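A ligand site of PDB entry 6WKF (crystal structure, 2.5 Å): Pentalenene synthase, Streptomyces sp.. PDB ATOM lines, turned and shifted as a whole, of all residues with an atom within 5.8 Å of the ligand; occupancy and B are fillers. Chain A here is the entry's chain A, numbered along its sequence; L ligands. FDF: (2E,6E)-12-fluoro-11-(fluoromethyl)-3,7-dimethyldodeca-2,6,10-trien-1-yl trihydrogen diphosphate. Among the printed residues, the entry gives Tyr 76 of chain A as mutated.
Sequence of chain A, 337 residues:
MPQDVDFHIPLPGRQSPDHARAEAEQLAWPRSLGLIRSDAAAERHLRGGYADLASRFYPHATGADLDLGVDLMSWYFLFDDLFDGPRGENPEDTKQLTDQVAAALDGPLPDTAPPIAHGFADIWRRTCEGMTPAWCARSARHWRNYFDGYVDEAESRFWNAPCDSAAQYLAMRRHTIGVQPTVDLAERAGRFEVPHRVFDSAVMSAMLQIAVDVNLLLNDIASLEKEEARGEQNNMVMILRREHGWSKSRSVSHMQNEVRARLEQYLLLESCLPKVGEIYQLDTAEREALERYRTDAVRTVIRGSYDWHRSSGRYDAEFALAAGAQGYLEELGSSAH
The guanidinium group (NH1) of Arg 173 is in salt-bridge range of an oxygen (O1A) of the ligand (2.9 Å). O3B of the ligand lies within hydrogen-bond range of ND2 of Asn 219. OG of Ser 223 lies within hydrogen-bond range of O3B of the ligand, 3.0 Å away.
The guanidinium group (NH2) of Arg 173 sits at hydrogen-bond distance from the side-chain hydroxyl (OG1) of Thr 176 (2.6 Å). OG of Ser 223 is in hydrogen-bond range of O of Asn 219, at 2.8 Å. ND2 of Asn 215 lies within hydrogen-bond range of O of Val 301 (3.1 Å). The side-chain hydroxyl (OG1) of Thr 182 sits at hydrogen-bond distance from the backbone carbonyl oxygen (O) of Gly 178 (2.9 Å). OH of Tyr 76 is in hydrogen-bond range of O of Gly 178 (2.8 Å). The side-chain hydroxyl (OG1) of Thr 182 sits at hydrogen-bond distance from the side-chain hydroxyl (OH) of Tyr 76. The side-chain amide oxygen (OD1) of Asn 215 lies within hydrogen-bond range of the side-chain hydroxyl (OG) of Ser 305, at 3.0 Å. The side-chain carboxylate (OD1) of Asp 80 is in hydrogen-bond range of the side-chain hydroxyl (OH) of Tyr 150 (2.8 Å).
The side-chain hydroxyl of Tyr 146 lies close to a fluorine (F1) of the ligand (3.0 Å). A fluorine (F1) of the ligand lies close to the side-chain hydroxyl of Tyr 150, at 3.0 Å. Merely in contact with the ligand: Ile 177 (3.2 Å), Asp 80 (3.3 Å), Trp 308 (3.5 Å), Phe 77 (3.6 Å), Thr 176 (3.6 Å), Tyr 76 (3.6 Å), Asn 215 (3.6 Å), Thr 182 (3.7 Å) and Val 179 (3.8 Å).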
ATOM      1  N   LEU A  53      11.297 -30.251  15.794  1.00  0.00           N
ATOM      2  CA  LEU A  53      11.777 -28.872  15.878  1.00  0.00           C
ATOM      3  C   LEU A  53      12.126 -28.506  17.317  1.00  0.00           C
ATOM      4  O   LEU A  53      13.183 -27.916  17.583  1.00  0.00           O
ATOM      5  CB  LEU A  53      10.713 -27.918  15.320  1.00  0.00           C
ATOM      6  CG  LEU A  53      10.967 -26.416  15.466  1.00  0.00           C
ATOM      7  CD1 LEU A  53      12.273 -26.010  14.790  1.00  0.00           C
ATOM      8  CD2 LEU A  53       9.801 -25.634  14.882  1.00  0.00           C
ATOM      9  N   PHE A  57      15.569 -26.981  18.979  1.00  0.00           N
ATOM     10  CA  PHE A  57      15.640 -25.749  19.764  1.00  0.00           C
ATOM     11  C   PHE A  57      16.135 -26.019  21.181  1.00  0.00           C
ATOM     12  O   PHE A  57      16.826 -25.170  21.762  1.00  0.00           O
ATOM     13  CB  PHE A  57      14.256 -25.076  19.828  1.00  0.00           C
ATOM     14  CG  PHE A  57      13.870 -24.304  18.593  1.00  0.00           C
ATOM     15  CD1 PHE A  57      14.833 -23.787  17.739  1.00  0.00           C
ATOM     16  CD2 PHE A  57      12.532 -24.072  18.295  1.00  0.00           C
ATOM     17  CE1 PHE A  57      14.480 -23.073  16.608  1.00  0.00           C
ATOM     18  CE2 PHE A  57      12.156 -23.358  17.162  1.00  0.00           C
ATOM     19  CZ  PHE A  57      13.127 -22.856  16.323  1.00  0.00           C
ATOM     20  N   MET A  73       5.827 -25.602  20.673  1.00  0.00           N
ATOM     21  CA  MET A  73       5.818 -25.687  19.211  1.00  0.00           C
ATOM     22  C   MET A  73       4.451 -26.121  18.703  1.00  0.00           C
ATOM     23  O   MET A  73       3.917 -25.548  17.752  1.00  0.00           O
ATOM     24  CB  MET A  73       6.903 -26.658  18.734  1.00  0.00           C
ATOM     25  CG  MET A  73       8.341 -26.222  19.054  1.00  0.00           C
ATOM     26  SD  MET A  73       8.763 -24.593  18.393  1.00  0.00           S
ATOM     27  CE  MET A  73       8.885 -23.651  19.913  1.00  0.00           C
ATOM     28  N   TYR A  76       2.155 -23.216  19.061  1.00  0.00           N
ATOM     29  CA  TYR A  76       2.468 -22.130  18.123  1.00  0.00           C
ATOM     30  C   TYR A  76       1.778 -22.317  16.785  1.00  0.00           C
ATOM     31  O   TYR A  76       1.230 -21.352  16.295  1.00  0.00           O
ATOM     32  CB  TYR A  76       3.951 -22.151  17.775  1.00  0.00           C
ATOM     33  CG  TYR A  76       4.799 -21.195  18.558  1.00  0.00           C
ATOM     34  CD1 TYR A  76       4.421 -19.889  18.713  1.00  0.00           C
ATOM     35  CD2 TYR A  76       5.985 -21.607  19.114  1.00  0.00           C
ATOM     36  CE1 TYR A  76       5.202 -18.999  19.436  1.00  0.00           C
ATOM     37  CE2 TYR A  76       6.776 -20.734  19.826  1.00  0.00           C
ATOM     38  CZ  TYR A  76       6.380 -19.422  19.992  1.00  0.00           C
ATOM     39  OH  TYR A  76       7.163 -18.571  20.684  1.00  0.00           O
ATOM     40  N   PHE A  77       1.816 -23.511  16.220  1.00  0.00           N
ATOM     41  CA  PHE A  77       1.265 -23.699  14.880  1.00  0.00           C
ATOM     42  C   PHE A  77      -0.242 -23.902  14.914  1.00  0.00           C
ATOM     43  O   PHE A  77      -0.929 -23.505  13.971  1.00  0.00           O
ATOM     44  CB  PHE A  77       1.988 -24.851  14.188  1.00  0.00           C
ATOM     45  CG  PHE A  77       3.421 -24.544  13.881  1.00  0.00           C
ATOM     46  CD1 PHE A  77       4.408 -24.744  14.835  1.00  0.00           C
ATOM     47  CD2 PHE A  77       3.780 -24.022  12.648  1.00  0.00           C
ATOM     48  CE1 PHE A  77       5.732 -24.440  14.563  1.00  0.00           C
ATOM     49  CE2 PHE A  77       5.100 -23.725  12.364  1.00  0.00           C
ATOM     50  CZ  PHE A  77       6.073 -23.932  13.326  1.00  0.00           C
ATOM     51  N   ASP A  80      -1.312 -20.098  15.247  1.00  0.00           N
ATOM     52  CA  ASP A  80      -1.181 -19.372  13.993  1.00  0.00           C
ATOM     53  C   ASP A  80      -2.225 -19.829  12.974  1.00  0.00           C
ATOM     54  O   ASP A  80      -2.620 -19.049  12.094  1.00  0.00           O
ATOM     55  CB  ASP A  80       0.231 -19.549  13.434  1.00  0.00           C
ATOM     56  CG  ASP A  80       0.503 -18.653  12.245  1.00  0.00           C
ATOM     57  OD1 ASP A  80       0.449 -17.411  12.409  1.00  0.00           O
ATOM     58  OD2 ASP A  80       0.781 -19.169  11.147  1.00  0.00           O
ATOM     59  N   TYR A 146       4.280 -10.486  21.476  1.00  0.00           N
ATOM     60  CA  TYR A 146       3.947 -11.430  20.420  1.00  0.00           C
ATOM     61  C   TYR A 146       2.486 -11.295  20.003  1.00  0.00           C
ATOM     62  O   TYR A 146       2.168 -11.220  18.818  1.00  0.00           O
ATOM     63  CB  TYR A 146       4.259 -12.848  20.908  1.00  0.00           C
ATOM     64  CG  TYR A 146       3.736 -13.980  20.051  1.00  0.00           C
ATOM     65  CD1 TYR A 146       4.381 -14.337  18.871  1.00  0.00           C
ATOM     66  CD2 TYR A 146       2.627 -14.700  20.436  1.00  0.00           C
ATOM     67  CE1 TYR A 146       3.920 -15.379  18.098  1.00  0.00           C
ATOM     68  CE2 TYR A 146       2.152 -15.749  19.670  1.00  0.00           C
ATOM     69  CZ  TYR A 146       2.801 -16.082  18.493  1.00  0.00           C
ATOM     70  OH  TYR A 146       2.321 -17.119  17.730  1.00  0.00           O
ATOM     71  N   TYR A 150       0.522  -9.770  16.419  1.00  0.00           N
ATOM     72  CA  TYR A 150      -0.544 -10.348  15.620  1.00  0.00           C
ATOM     73  C   TYR A 150      -1.618  -9.308  15.311  1.00  0.00           C
ATOM     74  O   TYR A 150      -2.123  -9.248  14.183  1.00  0.00           O
ATOM     75  CB  TYR A 150      -1.148 -11.563  16.334  1.00  0.00           C
ATOM     76  CG  TYR A 150      -0.476 -12.846  15.927  1.00  0.00           C
ATOM     77  CD1 TYR A 150       0.806 -13.147  16.394  1.00  0.00           C
ATOM     78  CD2 TYR A 150      -1.088 -13.746  15.058  1.00  0.00           C
ATOM     79  CE1 TYR A 150       1.443 -14.311  16.018  1.00  0.00           C
ATOM     80  CE2 TYR A 150      -0.461 -14.913  14.677  1.00  0.00           C
ATOM     81  CZ  TYR A 150       0.816 -15.190  15.167  1.00  0.00           C
ATOM     82  OH  TYR A 150       1.469 -16.350  14.800  1.00  0.00           O
ATOM     83  N   ARG A 173       7.382  -8.053  12.111  1.00  0.00           N
ATOM     84  CA  ARG A 173       7.720  -9.471  12.002  1.00  0.00           C
ATOM     85  C   ARG A 173       8.636  -9.916  13.133  1.00  0.00           C
ATOM     86  O   ARG A 173       8.603 -11.093  13.517  1.00  0.00           O
ATOM     87  CB  ARG A 173       8.377  -9.752  10.646  1.00  0.00           C
ATOM     88  CG  ARG A 173       8.471 -11.227  10.320  1.00  0.00           C
ATOM     89  CD  ARG A 173       7.083 -11.842  10.154  1.00  0.00           C
ATOM     90  NE  ARG A 173       7.159 -13.282   9.914  1.00  0.00           N
ATOM     91  CZ  ARG A 173       6.611 -14.198  10.701  1.00  0.00           C
ATOM     92  NH1 ARG A 173       6.736 -15.490  10.401  1.00  0.00           N
ATOM     93  NH2 ARG A 173       5.927 -13.840  11.777  1.00  0.00           N
ATOM     94  N   THR A 176       6.123 -11.166  15.750  1.00  0.00           N
ATOM     95  CA  THR A 176       5.216 -12.252  15.403  1.00  0.00           C
ATOM     96  C   THR A 176       5.930 -13.549  15.056  1.00  0.00           C
ATOM     97  O   THR A 176       5.300 -14.610  15.057  1.00  0.00           O
ATOM     98  CB  THR A 176       4.316 -11.847  14.239  1.00  0.00           C
ATOM     99  OG1 THR A 176       5.108 -11.727  13.043  1.00  0.00           O
ATOM    100  CG2 THR A 176       3.657 -10.524  14.530  1.00  0.00           C
ATOM    101  N   ILE A 177       7.229 -13.488  14.754  1.00  0.00           N
ATOM    102  CA  ILE A 177       7.996 -14.697  14.486  1.00  0.00           C
ATOM    103  C   ILE A 177       8.092 -15.575  15.733  1.00  0.00           C
ATOM    104  O   ILE A 177       8.278 -16.793  15.616  1.00  0.00           O
ATOM    105  CB  ILE A 177       9.394 -14.325  13.939  1.00  0.00           C
ATOM    106  CG1 ILE A 177      10.129 -15.561  13.429  1.00  0.00           C
ATOM    107  CG2 ILE A 177      10.198 -13.597  14.997  1.00  0.00           C
ATOM    108  CD1 ILE A 177       9.451 -16.247  12.260  1.00  0.00           C
ATOM    109  N   GLY A 178       7.952 -14.986  16.908  1.00  0.00           N
ATOM    110  CA  GLY A 178       7.904 -15.759  18.137  1.00  0.00           C
ATOM    111  C   GLY A 178       9.226 -16.353  18.565  1.00  0.00           C
ATOM    112  O   GLY A 178       9.258 -17.403  19.210  1.00  0.00           O
ATOM    113  N   VAL A 179      10.335 -15.703  18.218  1.00  0.00           N
ATOM    114  CA  VAL A 179      11.651 -16.240  18.560  1.00  0.00           C
ATOM    115  C   VAL A 179      11.967 -16.026  20.033  1.00  0.00           C
ATOM    116  O   VAL A 179      12.495 -16.916  20.705  1.00  0.00           O
ATOM    117  CB  VAL A 179      12.714 -15.624  17.639  1.00  0.00           C
ATOM    118  CG1 VAL A 179      14.106 -15.865  18.199  1.00  0.00           C
ATOM    119  CG2 VAL A 179      12.582 -16.204  16.246  1.00  0.00           C
ATOM    120  N   THR A 182      10.455 -18.482  22.348  1.00  0.00           N
ATOM    121  CA  THR A 182      11.179 -19.729  22.137  1.00  0.00           C
ATOM    122  C   THR A 182      12.493 -19.731  22.910  1.00  0.00           C
ATOM    123  O   THR A 182      12.820 -20.697  23.610  1.00  0.00           O
ATOM    124  CB  THR A 182      11.416 -19.945  20.644  1.00  0.00           C
ATOM    125  OG1 THR A 182      10.158 -20.083  19.969  1.00  0.00           O
ATOM    126  CG2 THR A 182      12.266 -21.184  20.406  1.00  0.00           C
ATOM    127  N   ASN A 215      15.869 -15.843  11.811  1.00  0.00           N
ATOM    128  CA  ASN A 215      14.758 -16.779  11.787  1.00  0.00           C
ATOM    129  C   ASN A 215      13.693 -16.357  10.782  1.00  0.00           C
ATOM    130  O   ASN A 215      13.181 -17.181  10.016  1.00  0.00           O
ATOM    131  CB  ASN A 215      14.145 -16.899  13.177  1.00  0.00           C
ATOM    132  CG  ASN A 215      14.697 -18.075  13.953  1.00  0.00           C
ATOM    133  OD1 ASN A 215      14.096 -19.140  13.989  1.00  0.00           O
ATOM    134  ND2 ASN A 215      15.851 -17.876  14.593  1.00  0.00           N
ATOM    135  N   ASN A 219      12.612 -18.120   7.239  1.00  0.00           N
ATOM    136  CA  ASN A 219      11.220 -18.515   7.124  1.00  0.00           C
ATOM    137  C   ASN A 219      10.570 -17.904   5.882  1.00  0.00           C
ATOM    138  O   ASN A 219       9.749 -18.554   5.227  1.00  0.00           O
ATOM    139  CB  ASN A 219      10.453 -18.115   8.385  1.00  0.00           C
ATOM    140  CG  ASN A 219       9.023 -18.594   8.368  1.00  0.00           C
ATOM    141  OD1 ASN A 219       8.731 -19.730   8.720  1.00  0.00           O
ATOM    142  ND2 ASN A 219       8.111 -17.720   7.938  1.00  0.00           N
ATOM    143  N   SER A 223       8.973 -19.941   2.842  1.00  0.00           N
ATOM    144  CA  SER A 223       7.560 -19.659   2.574  1.00  0.00           C
ATOM    145  C   SER A 223       7.341 -19.030   1.197  1.00  0.00           C
ATOM    146  O   SER A 223       6.226 -18.577   0.913  1.00  0.00           O
ATOM    147  CB  SER A 223       6.987 -18.741   3.659  1.00  0.00           C
ATOM    148  OG  SER A 223       7.050 -19.358   4.928  1.00  0.00           O
ATOM    149  N   VAL A 301      18.491 -21.519  18.883  1.00  0.00           N
ATOM    150  CA  VAL A 301      17.337 -20.922  18.144  1.00  0.00           C
ATOM    151  C   VAL A 301      17.792 -20.525  16.739  1.00  0.00           C
ATOM    152  O   VAL A 301      16.962 -20.491  15.858  1.00  0.00           O
ATOM    153  CB  VAL A 301      16.664 -19.781  18.901  1.00  0.00           C
ATOM    154  CG1 VAL A 301      17.589 -18.605  19.120  1.00  0.00           C
ATOM    155  CG2 VAL A 301      15.434 -19.295  18.186  1.00  0.00           C
ATOM    156  N   SER A 305      16.185 -23.804  13.664  1.00  0.00           N
ATOM    157  CA  SER A 305      15.244 -23.572  12.580  1.00  0.00           C
ATOM    158  C   SER A 305      15.848 -23.929  11.229  1.00  0.00           C
ATOM    159  O   SER A 305      15.147 -24.427  10.350  1.00  0.00           O
ATOM    160  CB  SER A 305      14.766 -22.119  12.605  1.00  0.00           C
ATOM    161  OG  SER A 305      15.852 -21.239  12.799  1.00  0.00           O
ATOM    162  N   TRP A 308      15.833 -27.638  10.810  1.00  0.00           N
ATOM    163  CA  TRP A 308      14.447 -28.083  10.686  1.00  0.00           C
ATOM    164  C   TRP A 308      13.964 -27.914   9.252  1.00  0.00           C
ATOM    165  O   TRP A 308      13.503 -28.872   8.617  1.00  0.00           O
ATOM    166  CB  TRP A 308      13.583 -27.317  11.675  1.00  0.00           C
ATOM    167  CG  TRP A 308      12.134 -27.726  11.726  1.00  0.00           C
ATOM    168  CD1 TRP A 308      11.630 -28.928  12.145  1.00  0.00           C
ATOM    169  CD2 TRP A 308      11.003 -26.912  11.396  1.00  0.00           C
ATOM    170  NE1 TRP A 308      10.258 -28.915  12.074  1.00  0.00           N
ATOM    171  CE2 TRP A 308       9.849 -27.682  11.622  1.00  0.00           C
ATOM    172  CE3 TRP A 308      10.853 -25.593  10.935  1.00  0.00           C
ATOM    173  CZ2 TRP A 308       8.565 -27.203  11.384  1.00  0.00           C
ATOM    174  CZ3 TRP A 308       9.586 -25.119  10.711  1.00  0.00           C
ATOM    175  CH2 TRP A 308       8.456 -25.916  10.927  1.00  0.00           C
ATOM    176  N   HIS A 309      14.062 -26.693   8.717  1.00  0.00           N
ATOM    177  CA  HIS A 309      13.746 -26.428   7.314  1.00  0.00           C
ATOM    178  C   HIS A 309      14.631 -27.272   6.392  1.00  0.00           C
ATOM    179  O   HIS A 309      14.264 -28.379   5.989  1.00  0.00           O
ATOM    180  CB  HIS A 309      13.912 -24.941   6.981  1.00  0.00           C
ATOM    181  CG  HIS A 309      13.012 -24.036   7.743  1.00  0.00           C
ATOM    182  ND1 HIS A 309      13.396 -23.407   8.908  1.00  0.00           N
ATOM    183  CD2 HIS A 309      11.747 -23.617   7.497  1.00  0.00           C
ATOM    184  CE1 HIS A 309      12.407 -22.656   9.356  1.00  0.00           C
ATOM    185  NE2 HIS A 309      11.385 -22.768   8.520  1.00  0.00           N
HETATM  186  PA  FDF L   1       4.709 -18.122  10.141  1.00  0.00           P
HETATM  187  PB  FDF L   1       4.657 -20.279   8.296  1.00  0.00           P
HETATM  188  C1  FDF L   1       6.621 -19.510  11.296  1.00  0.00           C
HETATM  189  O1  FDF L   1       6.257 -18.345  10.543  1.00  0.00           O
HETATM  190  O1A FDF L   1       4.635 -17.051   9.066  1.00  0.00           O
HETATM  191  O1B FDF L   1       3.516 -20.666   7.386  1.00  0.00           O
HETATM  192  C2  FDF L   1       8.067 -19.507  11.759  1.00  0.00           C
HETATM  193  O2A FDF L   1       3.933 -17.662  11.365  1.00  0.00           O
HETATM  194  O2B FDF L   1       5.365 -21.530   8.781  1.00  0.00           O
HETATM  195  C3  FDF L   1       8.849 -20.622  11.776  1.00  0.00           C
HETATM  196  O3A FDF L   1       4.047 -19.479   9.563  1.00  0.00           O
HETATM  197  O3B FDF L   1       5.629 -19.388   7.549  1.00  0.00           O
HETATM  198  C4  FDF L   1       8.248 -21.943  11.309  1.00  0.00           C
HETATM  199  C5  FDF L   1      10.280 -20.454  12.273  1.00  0.00           C
HETATM  200  C6  FDF L   1      10.656 -21.402  13.414  1.00  0.00           C
HETATM  201  C7  FDF L   1       9.663 -21.384  14.549  1.00  0.00           C
HETATM  202  C8  FDF L   1       9.765 -20.546  15.617  1.00  0.00           C
HETATM  203  C9  FDF L   1       8.649 -20.660  16.652  1.00  0.00           C
HETATM  204  C10 FDF L   1      10.919 -19.560  15.733  1.00  0.00           C
HETATM  205  C11 FDF L   1       7.452 -19.756  16.362  1.00  0.00           C
HETATM  206  C12 FDF L   1       6.471 -20.432  15.422  1.00  0.00           C
HETATM  207  C13 FDF L   1       5.417 -19.782  14.890  1.00  0.00           C
HETATM  208  C14 FDF L   1       4.459 -20.512  13.955  1.00  0.00           C
HETATM  209  C15 FDF L   1       5.230 -18.323  15.270  1.00  0.00           C
HETATM  210  F1  FDF L   1       3.922 -17.918  15.277  1.00  0.00           F
HETATM  211  F2  FDF L   1       3.526 -19.661  13.420  1.00  0.00           F
